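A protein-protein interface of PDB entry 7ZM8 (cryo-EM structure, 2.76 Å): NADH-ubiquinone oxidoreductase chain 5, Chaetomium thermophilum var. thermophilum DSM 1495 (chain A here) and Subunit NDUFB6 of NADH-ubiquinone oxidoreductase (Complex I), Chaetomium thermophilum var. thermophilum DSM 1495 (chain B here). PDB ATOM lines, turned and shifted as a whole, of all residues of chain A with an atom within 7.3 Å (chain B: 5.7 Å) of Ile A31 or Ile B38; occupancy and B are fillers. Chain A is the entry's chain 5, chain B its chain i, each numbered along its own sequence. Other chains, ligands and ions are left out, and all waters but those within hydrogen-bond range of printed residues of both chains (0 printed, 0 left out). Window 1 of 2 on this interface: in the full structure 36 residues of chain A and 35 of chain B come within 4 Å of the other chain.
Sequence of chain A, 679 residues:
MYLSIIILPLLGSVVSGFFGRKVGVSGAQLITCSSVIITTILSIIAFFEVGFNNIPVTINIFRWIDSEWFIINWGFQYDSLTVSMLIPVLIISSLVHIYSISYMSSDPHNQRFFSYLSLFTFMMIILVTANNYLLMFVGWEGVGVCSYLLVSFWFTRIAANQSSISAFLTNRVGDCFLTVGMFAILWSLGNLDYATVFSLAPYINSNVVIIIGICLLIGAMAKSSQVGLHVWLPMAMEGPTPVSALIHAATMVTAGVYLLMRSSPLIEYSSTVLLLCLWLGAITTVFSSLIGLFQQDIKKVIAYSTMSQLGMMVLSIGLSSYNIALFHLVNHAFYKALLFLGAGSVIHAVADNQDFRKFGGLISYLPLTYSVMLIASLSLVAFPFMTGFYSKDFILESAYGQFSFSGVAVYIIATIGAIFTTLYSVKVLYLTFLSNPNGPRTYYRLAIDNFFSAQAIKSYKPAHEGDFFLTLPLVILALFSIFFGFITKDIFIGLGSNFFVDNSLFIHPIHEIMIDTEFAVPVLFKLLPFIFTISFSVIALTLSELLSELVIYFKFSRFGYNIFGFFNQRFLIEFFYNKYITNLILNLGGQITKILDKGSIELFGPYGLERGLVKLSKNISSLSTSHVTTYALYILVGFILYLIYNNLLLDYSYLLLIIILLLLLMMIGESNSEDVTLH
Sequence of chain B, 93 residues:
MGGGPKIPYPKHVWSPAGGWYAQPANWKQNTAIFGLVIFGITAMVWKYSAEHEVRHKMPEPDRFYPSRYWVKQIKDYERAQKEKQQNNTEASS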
ATOM      1  N   ILE A   7       9.998  18.127  -9.149  1.00  0.00           N
ATOM      2  CA  ILE A   7       8.566  18.359  -8.981  1.00  0.00           C
ATOM      3  C   ILE A   7       7.996  17.633  -7.763  1.00  0.00           C
ATOM      4  O   ILE A   7       7.076  18.146  -7.122  1.00  0.00           O
ATOM      5  CB  ILE A   7       7.802  17.983 -10.268  1.00  0.00           C
ATOM      6  CG1 ILE A   7       6.370  18.514 -10.224  1.00  0.00           C
ATOM      7  CG2 ILE A   7       7.732  16.486 -10.450  1.00  0.00           C
ATOM      8  CD1 ILE A   7       6.279  20.011 -10.237  1.00  0.00           C
ATOM      9  N   LEU A   8       8.508  16.446  -7.417  1.00  0.00           N
ATOM     10  CA  LEU A   8       7.869  15.645  -6.369  1.00  0.00           C
ATOM     11  C   LEU A   8       7.844  16.306  -5.000  1.00  0.00           C
ATOM     12  O   LEU A   8       6.767  16.334  -4.382  1.00  0.00           O
ATOM     13  CB  LEU A   8       8.519  14.263  -6.275  1.00  0.00           C
ATOM     14  CG  LEU A   8       8.312  13.288  -7.422  1.00  0.00           C
ATOM     15  CD1 LEU A   8       9.137  12.049  -7.194  1.00  0.00           C
ATOM     16  CD2 LEU A   8       6.847  12.936  -7.496  1.00  0.00           C
ATOM     17  N   LEU A  10       7.702  19.305  -4.210  1.00  0.00           N
ATOM     18  CA  LEU A  10       6.775  20.427  -4.269  1.00  0.00           C
ATOM     19  C   LEU A  10       5.328  19.969  -4.133  1.00  0.00           C
ATOM     20  O   LEU A  10       4.526  20.627  -3.465  1.00  0.00           O
ATOM     21  CB  LEU A  10       6.978  21.184  -5.577  1.00  0.00           C
ATOM     22  CG  LEU A  10       6.030  22.329  -5.902  1.00  0.00           C
ATOM     23  CD1 LEU A  10       6.307  23.537  -5.033  1.00  0.00           C
ATOM     24  CD2 LEU A  10       6.155  22.665  -7.363  1.00  0.00           C
ATOM     25  N   LEU A  11       4.971  18.855  -4.770  1.00  0.00           N
ATOM     26  CA  LEU A  11       3.591  18.384  -4.730  1.00  0.00           C
ATOM     27  C   LEU A  11       3.210  17.892  -3.343  1.00  0.00           C
ATOM     28  O   LEU A  11       2.101  18.165  -2.867  1.00  0.00           O
ATOM     29  CB  LEU A  11       3.387  17.281  -5.763  1.00  0.00           C
ATOM     30  CG  LEU A  11       3.895  17.637  -7.156  1.00  0.00           C
ATOM     31  CD1 LEU A  11       3.672  16.488  -8.119  1.00  0.00           C
ATOM     32  CD2 LEU A  11       3.239  18.907  -7.653  1.00  0.00           C
ATOM     33  N   GLY A  12       4.110  17.166  -2.678  1.00  0.00           N
ATOM     34  CA  GLY A  12       3.833  16.716  -1.327  1.00  0.00           C
ATOM     35  C   GLY A  12       3.669  17.858  -0.350  1.00  0.00           C
ATOM     36  O   GLY A  12       2.892  17.760   0.601  1.00  0.00           O
ATOM     37  N   SER A  13       4.406  18.946  -0.559  1.00  0.00           N
ATOM     38  CA  SER A  13       4.255  20.129   0.280  1.00  0.00           C
ATOM     39  C   SER A  13       2.875  20.747   0.114  1.00  0.00           C
ATOM     40  O   SER A  13       2.268  21.196   1.090  1.00  0.00           O
ATOM     41  CB  SER A  13       5.342  21.143  -0.064  1.00  0.00           C
ATOM     42  OG  SER A  13       5.213  22.322   0.706  1.00  0.00           O
ATOM     43  N   VAL A  15       0.021  19.299  -0.891  1.00  0.00           N
ATOM     44  CA  VAL A  15      -1.016  18.467  -0.294  1.00  0.00           C
ATOM     45  C   VAL A  15      -1.026  18.623   1.220  1.00  0.00           C
ATOM     46  O   VAL A  15      -2.088  18.759   1.834  1.00  0.00           O
ATOM     47  CB  VAL A  15      -0.834  16.997  -0.712  1.00  0.00           C
ATOM     48  CG1 VAL A  15      -1.915  16.135  -0.086  1.00  0.00           C
ATOM     49  CG2 VAL A  15      -0.856  16.869  -2.219  1.00  0.00           C
ATOM     50  N   SER A  16       0.149  18.610   1.847  1.00  0.00           N
ATOM     51  CA  SER A  16       0.208  18.707   3.300  1.00  0.00           C
ATOM     52  C   SER A  16      -0.211  20.085   3.802  1.00  0.00           C
ATOM     53  O   SER A  16      -0.759  20.201   4.902  1.00  0.00           O
ATOM     54  CB  SER A  16       1.614  18.372   3.783  1.00  0.00           C
ATOM     55  OG  SER A  16       1.672  18.348   5.196  1.00  0.00           O
ATOM     56  N   VAL A  23      -6.235  14.957   4.239  1.00  0.00           N
ATOM     57  CA  VAL A  23      -5.332  13.780   4.391  1.00  0.00           C
ATOM     58  C   VAL A  23      -5.065  13.485   5.870  1.00  0.00           C
ATOM     59  O   VAL A  23      -4.710  12.342   6.178  1.00  0.00           O
ATOM     60  CB  VAL A  23      -4.031  13.985   3.598  1.00  0.00           C
ATOM     61  CG1 VAL A  23      -4.254  13.843   2.105  1.00  0.00           C
ATOM     62  CG2 VAL A  23      -3.357  15.306   3.921  1.00  0.00           C
ATOM     63  N   VAL A  25      -3.121  13.927   9.758  1.00  0.00           N
ATOM     64  CA  VAL A  25      -1.700  13.851  10.191  1.00  0.00           C
ATOM     65  C   VAL A  25      -1.053  12.644   9.519  1.00  0.00           C
ATOM     66  O   VAL A  25       0.045  12.791   8.983  1.00  0.00           O
ATOM     67  CB  VAL A  25      -1.636  13.735  11.724  1.00  0.00           C
ATOM     68  CG1 VAL A  25      -0.214  13.563  12.226  1.00  0.00           C
ATOM     69  CG2 VAL A  25      -2.331  14.893  12.419  1.00  0.00           C
ATOM     70  N   SER A  26      -1.739  11.504   9.526  1.00  0.00           N
ATOM     71  CA  SER A  26      -1.187  10.261   8.941  1.00  0.00           C
ATOM     72  C   SER A  26      -0.995  10.447   7.437  1.00  0.00           C
ATOM     73  O   SER A  26       0.091  10.121   6.949  1.00  0.00           O
ATOM     74  CB  SER A  26      -2.069   9.096   9.275  1.00  0.00           C
ATOM     75  OG  SER A  26      -2.143   8.902  10.677  1.00  0.00           O
ATOM     76  N   GLY A  27      -2.032  10.906   6.732  1.00  0.00           N
ATOM     77  CA  GLY A  27      -1.938  11.048   5.291  1.00  0.00           C
ATOM     78  C   GLY A  27      -0.923  12.085   4.869  1.00  0.00           C
ATOM     79  O   GLY A  27      -0.242  11.919   3.855  1.00  0.00           O
ATOM     80  N   ALA A  28      -0.824  13.181   5.621  1.00  0.00           N
ATOM     81  CA  ALA A  28       0.205  14.173   5.337  1.00  0.00           C
ATOM     82  C   ALA A  28       1.595  13.596   5.548  1.00  0.00           C
ATOM     83  O   ALA A  28       2.491  13.811   4.729  1.00  0.00           O
ATOM     84  CB  ALA A  28       0.003  15.409   6.207  1.00  0.00           C
ATOM     85  N   GLN A  29       1.790  12.847   6.632  1.00  0.00           N
ATOM     86  CA  GLN A  29       3.095  12.251   6.886  1.00  0.00           C
ATOM     87  C   GLN A  29       3.460  11.258   5.798  1.00  0.00           C
ATOM     88  O   GLN A  29       4.614  11.195   5.368  1.00  0.00           O
ATOM     89  CB  GLN A  29       3.112  11.569   8.253  1.00  0.00           C
ATOM     90  CG  GLN A  29       3.302  12.500   9.428  1.00  0.00           C
ATOM     91  CD  GLN A  29       3.035  11.808  10.743  1.00  0.00           C
ATOM     92  OE1 GLN A  29       2.536  10.687  10.772  1.00  0.00           O
ATOM     93  NE2 GLN A  29       3.374  12.466  11.842  1.00  0.00           N
ATOM     94  N   LEU A  30       2.490  10.470   5.343  1.00  0.00           N
ATOM     95  CA  LEU A  30       2.767   9.450   4.341  1.00  0.00           C
ATOM     96  C   LEU A  30       3.106  10.068   2.989  1.00  0.00           C
ATOM     97  O   LEU A  30       4.086   9.677   2.348  1.00  0.00           O
ATOM     98  CB  LEU A  30       1.569   8.513   4.229  1.00  0.00           C
ATOM     99  CG  LEU A  30       1.586   7.488   3.108  1.00  0.00           C
ATOM    100  CD1 LEU A  30       2.445   6.314   3.496  1.00  0.00           C
ATOM    101  CD2 LEU A  30       0.178   7.045   2.809  1.00  0.00           C
ATOM    102  N   ILE A  31       2.308  11.033   2.535  1.00  0.00           N
ATOM    103  CA  ILE A  31       2.553  11.641   1.231  1.00  0.00           C
ATOM    104  C   ILE A  31       3.828  12.476   1.248  1.00  0.00           C
ATOM    105  O   ILE A  31       4.615  12.453   0.296  1.00  0.00           O
ATOM    106  CB  ILE A  31       1.327  12.465   0.796  1.00  0.00           C
ATOM    107  CG1 ILE A  31       0.191  11.535   0.366  1.00  0.00           C
ATOM    108  CG2 ILE A  31       1.679  13.442  -0.301  1.00  0.00           C
ATOM    109  CD1 ILE A  31      -1.127  12.229   0.162  1.00  0.00           C
ATOM    110  N   THR A  32       4.048  13.232   2.321  1.00  0.00           N
ATOM    111  CA  THR A  32       5.265  14.028   2.434  1.00  0.00           C
ATOM    112  C   THR A  32       6.505  13.144   2.479  1.00  0.00           C
ATOM    113  O   THR A  32       7.494  13.405   1.784  1.00  0.00           O
ATOM    114  CB  THR A  32       5.182  14.921   3.672  1.00  0.00           C
ATOM    115  OG1 THR A  32       4.240  15.972   3.441  1.00  0.00           O
ATOM    116  CG2 THR A  32       6.511  15.506   4.007  1.00  0.00           C
ATOM    117  N   CYS A  33       6.476  12.092   3.294  1.00  0.00           N
ATOM    118  CA  CYS A  33       7.652  11.241   3.413  1.00  0.00           C
ATOM    119  C   CYS A  33       7.876  10.432   2.147  1.00  0.00           C
ATOM    120  O   CYS A  33       9.006  10.327   1.668  1.00  0.00           O
ATOM    121  CB  CYS A  33       7.526  10.323   4.627  1.00  0.00           C
ATOM    122  SG  CYS A  33       7.722  11.163   6.210  1.00  0.00           S
ATOM    123  N   SER A  34       6.813   9.873   1.574  1.00  0.00           N
ATOM    124  CA  SER A  34       6.979   9.030   0.396  1.00  0.00           C
ATOM    125  C   SER A  34       7.482   9.829  -0.803  1.00  0.00           C
ATOM    126  O   SER A  34       8.316   9.334  -1.566  1.00  0.00           O
ATOM    127  CB  SER A  34       5.671   8.307   0.070  1.00  0.00           C
ATOM    128  OG  SER A  34       4.585   9.203  -0.054  1.00  0.00           O
ATOM    129  N   SER A  35       7.001  11.060  -0.989  1.00  0.00           N
ATOM    130  CA  SER A  35       7.436  11.833  -2.148  1.00  0.00           C
ATOM    131  C   SER A  35       8.926  12.137  -2.082  1.00  0.00           C
ATOM    132  O   SER A  35       9.614  12.122  -3.107  1.00  0.00           O
ATOM    133  CB  SER A  35       6.644  13.134  -2.271  1.00  0.00           C
ATOM    134  OG  SER A  35       6.920  14.011  -1.196  1.00  0.00           O
ATOM    135  N   VAL A  36       9.444  12.424  -0.887  1.00  0.00           N
ATOM    136  CA  VAL A  36      10.868  12.719  -0.771  1.00  0.00           C
ATOM    137  C   VAL A  36      11.700  11.441  -0.759  1.00  0.00           C
ATOM    138  O   VAL A  36      12.876  11.481  -1.139  1.00  0.00           O
ATOM    139  CB  VAL A  36      11.147  13.591   0.471  1.00  0.00           C
ATOM    140  CG1 VAL A  36      10.838  12.851   1.755  1.00  0.00           C
ATOM    141  CG2 VAL A  36      12.559  14.132   0.465  1.00  0.00           C
ATOM    142  N   ILE A  37      11.125  10.301  -0.362  1.00  0.00           N
ATOM    143  CA  ILE A  37      11.828   9.028  -0.517  1.00  0.00           C
ATOM    144  C   ILE A  37      11.980   8.680  -1.991  1.00  0.00           C
ATOM    145  O   ILE A  37      13.046   8.238  -2.432  1.00  0.00           O
ATOM    146  CB  ILE A  37      11.112   7.896   0.245  1.00  0.00           C
ATOM    147  CG1 ILE A  37      11.038   8.178   1.745  1.00  0.00           C
ATOM    148  CG2 ILE A  37      11.823   6.580   0.024  1.00  0.00           C
ATOM    149  CD1 ILE A  37      12.362   8.290   2.415  1.00  0.00           C
ATOM    150  N   ILE A  38      10.915   8.866  -2.772  1.00  0.00           N
ATOM    151  CA  ILE A  38      10.968   8.591  -4.205  1.00  0.00           C
ATOM    152  C   ILE A  38      11.973   9.508  -4.883  1.00  0.00           C
ATOM    153  O   ILE A  38      12.752   9.076  -5.740  1.00  0.00           O
ATOM    154  CB  ILE A  38       9.567   8.740  -4.820  1.00  0.00           C
ATOM    155  CG1 ILE A  38       8.613   7.716  -4.220  1.00  0.00           C
ATOM    156  CG2 ILE A  38       9.620   8.566  -6.326  1.00  0.00           C
ATOM    157  CD1 ILE A  38       7.169   7.966  -4.577  1.00  0.00           C
ATOM    158  N   SER A 118       8.901  19.617   3.293  1.00  0.00           N
ATOM    159  CA  SER A 118       8.922  19.402   1.851  1.00  0.00           C
ATOM    160  C   SER A 118       9.183  20.691   1.088  1.00  0.00           C
ATOM    161  O   SER A 118       9.817  20.663   0.031  1.00  0.00           O
ATOM    162  CB  SER A 118       7.612  18.776   1.388  1.00  0.00           C
ATOM    163  OG  SER A 118       7.536  17.423   1.768  1.00  0.00           O
ATOM    164  N   THR B  31      -6.237  10.260   1.072  1.00  0.00           N
ATOM    165  CA  THR B  31      -4.771  10.119   0.867  1.00  0.00           C
ATOM    166  C   THR B  31      -4.515   9.256  -0.350  1.00  0.00           C
ATOM    167  O   THR B  31      -3.594   9.589  -1.111  1.00  0.00           O
ATOM    168  CB  THR B  31      -4.076   9.519   2.086  1.00  0.00           C
ATOM    169  OG1 THR B  31      -4.297  10.449   3.142  1.00  0.00           O
ATOM    170  CG2 THR B  31      -2.593   9.299   1.898  1.00  0.00           C
ATOM    171  N   ILE B  33      -6.516   9.090  -2.953  1.00  0.00           N
ATOM    172  CA  ILE B  33      -6.889   9.901  -4.109  1.00  0.00           C
ATOM    173  C   ILE B  33      -5.820  10.940  -4.408  1.00  0.00           C
ATOM    174  O   ILE B  33      -5.482  11.185  -5.571  1.00  0.00           O
ATOM    175  CB  ILE B  33      -8.265  10.546  -3.878  1.00  0.00           C
ATOM    176  CG1 ILE B  33      -9.317   9.462  -3.650  1.00  0.00           C
ATOM    177  CG2 ILE B  33      -8.644  11.443  -5.033  1.00  0.00           C
ATOM    178  CD1 ILE B  33      -9.480   8.525  -4.817  1.00  0.00           C
ATOM    179  N   PHE B  34      -5.277  11.575  -3.369  1.00  0.00           N
ATOM    180  CA  PHE B  34      -4.200  12.535  -3.575  1.00  0.00           C
ATOM    181  C   PHE B  34      -2.946  11.862  -4.105  1.00  0.00           C
ATOM    182  O   PHE B  34      -2.153  12.497  -4.803  1.00  0.00           O
ATOM    183  CB  PHE B  34      -3.898  13.274  -2.275  1.00  0.00           C
ATOM    184  CG  PHE B  34      -4.684  14.529  -2.107  1.00  0.00           C
ATOM    185  CD1 PHE B  34      -4.632  15.520  -3.063  1.00  0.00           C
ATOM    186  CD2 PHE B  34      -5.482  14.720  -0.998  1.00  0.00           C
ATOM    187  CE1 PHE B  34      -5.356  16.680  -2.915  1.00  0.00           C
ATOM    188  CE2 PHE B  34      -6.210  15.878  -0.845  1.00  0.00           C
ATOM    189  CZ  PHE B  34      -6.151  16.856  -1.807  1.00  0.00           C
ATOM    190  N   GLY B  35      -2.739  10.592  -3.772  1.00  0.00           N
ATOM    191  CA  GLY B  35      -1.593   9.881  -4.312  1.00  0.00           C
ATOM    192  C   GLY B  35      -1.696   9.669  -5.808  1.00  0.00           C
ATOM    193  O   GLY B  35      -0.707   9.807  -6.531  1.00  0.00           O
ATOM    194  N   LEU B  36      -2.889   9.327  -6.294  1.00  0.00           N
ATOM    195  CA  LEU B  36      -3.076   9.126  -7.725  1.00  0.00           C
ATOM    196  C   LEU B  36      -2.880  10.418  -8.504  1.00  0.00           C
ATOM    197  O   LEU B  36      -2.245  10.418  -9.562  1.00  0.00           O
ATOM    198  CB  LEU B  36      -4.458   8.541  -8.001  1.00  0.00           C
ATOM    199  CG  LEU B  36      -4.538   7.018  -8.072  1.00  0.00           C
ATOM    200  CD1 LEU B  36      -4.415   6.399  -6.692  1.00  0.00           C
ATOM    201  CD2 LEU B  36      -5.832   6.587  -8.744  1.00  0.00           C
ATOM    202  N   VAL B  37      -3.424  11.529  -8.008  1.00  0.00           N
ATOM    203  CA  VAL B  37      -3.265  12.790  -8.720  1.00  0.00           C
ATOM    204  C   VAL B  37      -1.807  13.236  -8.694  1.00  0.00           C
ATOM    205  O   VAL B  37      -1.310  13.820  -9.664  1.00  0.00           O
ATOM    206  CB  VAL B  37      -4.216  13.862  -8.157  1.00  0.00           C
ATOM    207  CG1 VAL B  37      -3.825  14.274  -6.763  1.00  0.00           C
ATOM    208  CG2 VAL B  37      -4.249  15.072  -9.077  1.00  0.00           C
ATOM    209  N   ILE B  38      -1.093  12.962  -7.599  1.00  0.00           N
ATOM    210  CA  ILE B  38       0.351  13.176  -7.590  1.00  0.00           C
ATOM    211  C   ILE B  38       1.013  12.305  -8.648  1.00  0.00           C
ATOM    212  O   ILE B  38       1.817  12.781  -9.457  1.00  0.00           O
ATOM    213  CB  ILE B  38       0.932  12.904  -6.190  1.00  0.00           C
ATOM    214  CG1 ILE B  38       0.617  14.055  -5.242  1.00  0.00           C
ATOM    215  CG2 ILE B  38       2.429  12.720  -6.251  1.00  0.00           C
ATOM    216  CD1 ILE B  38       1.325  13.957  -3.912  1.00  0.00           C
ATOM    217  N   PHE B  39       0.663  11.018  -8.670  1.00  0.00           N
ATOM    218  CA  PHE B  39       1.245  10.095  -9.637  1.00  0.00           C
ATOM    219  C   PHE B  39       0.894  10.506 -11.061  1.00  0.00           C
ATOM    220  O   PHE B  39       1.723  10.392 -11.969  1.00  0.00           O
ATOM    221  CB  PHE B  39       0.776   8.668  -9.324  1.00  0.00           C
ATOM    222  CG  PHE B  39       1.186   7.627 -10.343  1.00  0.00           C
ATOM    223  CD1 PHE B  39       0.560   7.536 -11.580  1.00  0.00           C
ATOM    224  CD2 PHE B  39       2.138   6.677 -10.018  1.00  0.00           C
ATOM    225  CE1 PHE B  39       0.930   6.570 -12.491  1.00  0.00           C
ATOM    226  CE2 PHE B  39       2.512   5.709 -10.926  1.00  0.00           C
ATOM    227  CZ  PHE B  39       1.903   5.653 -12.162  1.00  0.00           C
ATOM    228  N   GLY B  40      -0.334  10.969 -11.280  1.00  0.00           N
ATOM    229  CA  GLY B  40      -0.712  11.432 -12.604  1.00  0.00           C
ATOM    230  C   GLY B  40       0.007  12.702 -13.015  1.00  0.00           C
ATOM    231  O   GLY B  40       0.424  12.839 -14.167  1.00  0.00           O
ATOM    232  N   ILE B  41       0.144  13.652 -12.092  1.00  0.00           N
ATOM    233  CA  ILE B  41       0.857  14.887 -12.404  1.00  0.00           C
ATOM    234  C   ILE B  41       2.324  14.597 -12.676  1.00  0.00           C
ATOM    235  O   ILE B  41       2.903  15.100 -13.644  1.00  0.00           O
ATOM    236  CB  ILE B  41       0.692  15.911 -11.268  1.00  0.00           C
ATOM    237  CG1 ILE B  41      -0.697  16.542 -11.302  1.00  0.00           C
ATOM    238  CG2 ILE B  41       1.766  16.988 -11.361  1.00  0.00           C
ATOM    239  CD1 ILE B  41      -0.933  17.516 -10.182  1.00  0.00           C
ATOM    240  N   THR B  42       2.949  13.774 -11.832  1.00  0.00           N
ATOM    241  CA  THR B  42       4.363  13.489 -12.018  1.00  0.00           C
ATOM    242  C   THR B  42       4.600  12.621 -13.243  1.00  0.00           C
ATOM    243  O   THR B  42       5.742  12.502 -13.696  1.00  0.00           O
ATOM    244  CB  THR B  42       4.950  12.821 -10.776  1.00  0.00           C
ATOM    245  OG1 THR B  42       6.370  12.720 -10.917  1.00  0.00           O
ATOM    246  CG2 THR B  42       4.411  11.428 -10.637  1.00  0.00           C
ATOM    247  N   ALA B  43       3.544  12.004 -13.779  1.00  0.00           N
ATOM    248  CA  ALA B  43       3.656  11.257 -15.024  1.00  0.00           C
ATOM    249  C   ALA B  43       3.717  12.184 -16.231  1.00  0.00           C
ATOM    250  O   ALA B  43       4.328  11.841 -17.247  1.00  0.00           O
ATOM    251  CB  ALA B  43       2.484  10.288 -15.152  1.00  0.00           C
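Among the printed residues, merely in contact across the chains: Gly A27 with Thr B31, Val A23 with Phe B34, Leu A8 with Thr B42, Val A23 with Thr B31, Ile A31 with Ile B38, Leu A30 with Thr B31, Ile A31 with Thr B31, Val A15 with Phe B34, Leu A11 with Ile B41 and Ile A31 with Phe B34.
Ile A31 touches three residues of chain B. Printed residues of chain A within 4 Å of Ile B38: Ile A31. Of the printed residues of chain B, Gly A27 touches Thr B31 (3.2 Å). Of the printed residues of chain B, Val A15 touches Phe B34 (3.8 Å). Of the printed residues of chain A, Thr B31 touches Val A23 (3.5 Å), Gly A27 (3.2 Å), Leu A30 (3.7 Å) and Ile A31 (3.7 Å). Phe B39 touches none of the printed residues of chain A. Gly A12 touches none of the printed residues of chain B.
Hydrophobic or aromatic side chains of chain A that line the printed part of chain B: Leu A8, Leu A11, Val A15, Val A23, Leu A30 and Ile A31. Of the 12 printed residues of chain B, 5 touch a printed residue of chain A. Printed residues of chain B that touch a printed residue of chain A: Thr B31, Phe B34, Ile B38, Ile B41 and Thr B42. Among the printed residues, 10 pairs touch across the chains.
OG of Ser A34 sits at hydrogen-bond distance from O of Leu A30 (2.5 Å). OG of Ser A35 sits at hydrogen-bond distance from O of Ile A31. OG of Ser A34 lies within hydrogen-bond range of O of Ile A31 (3.3 Å).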
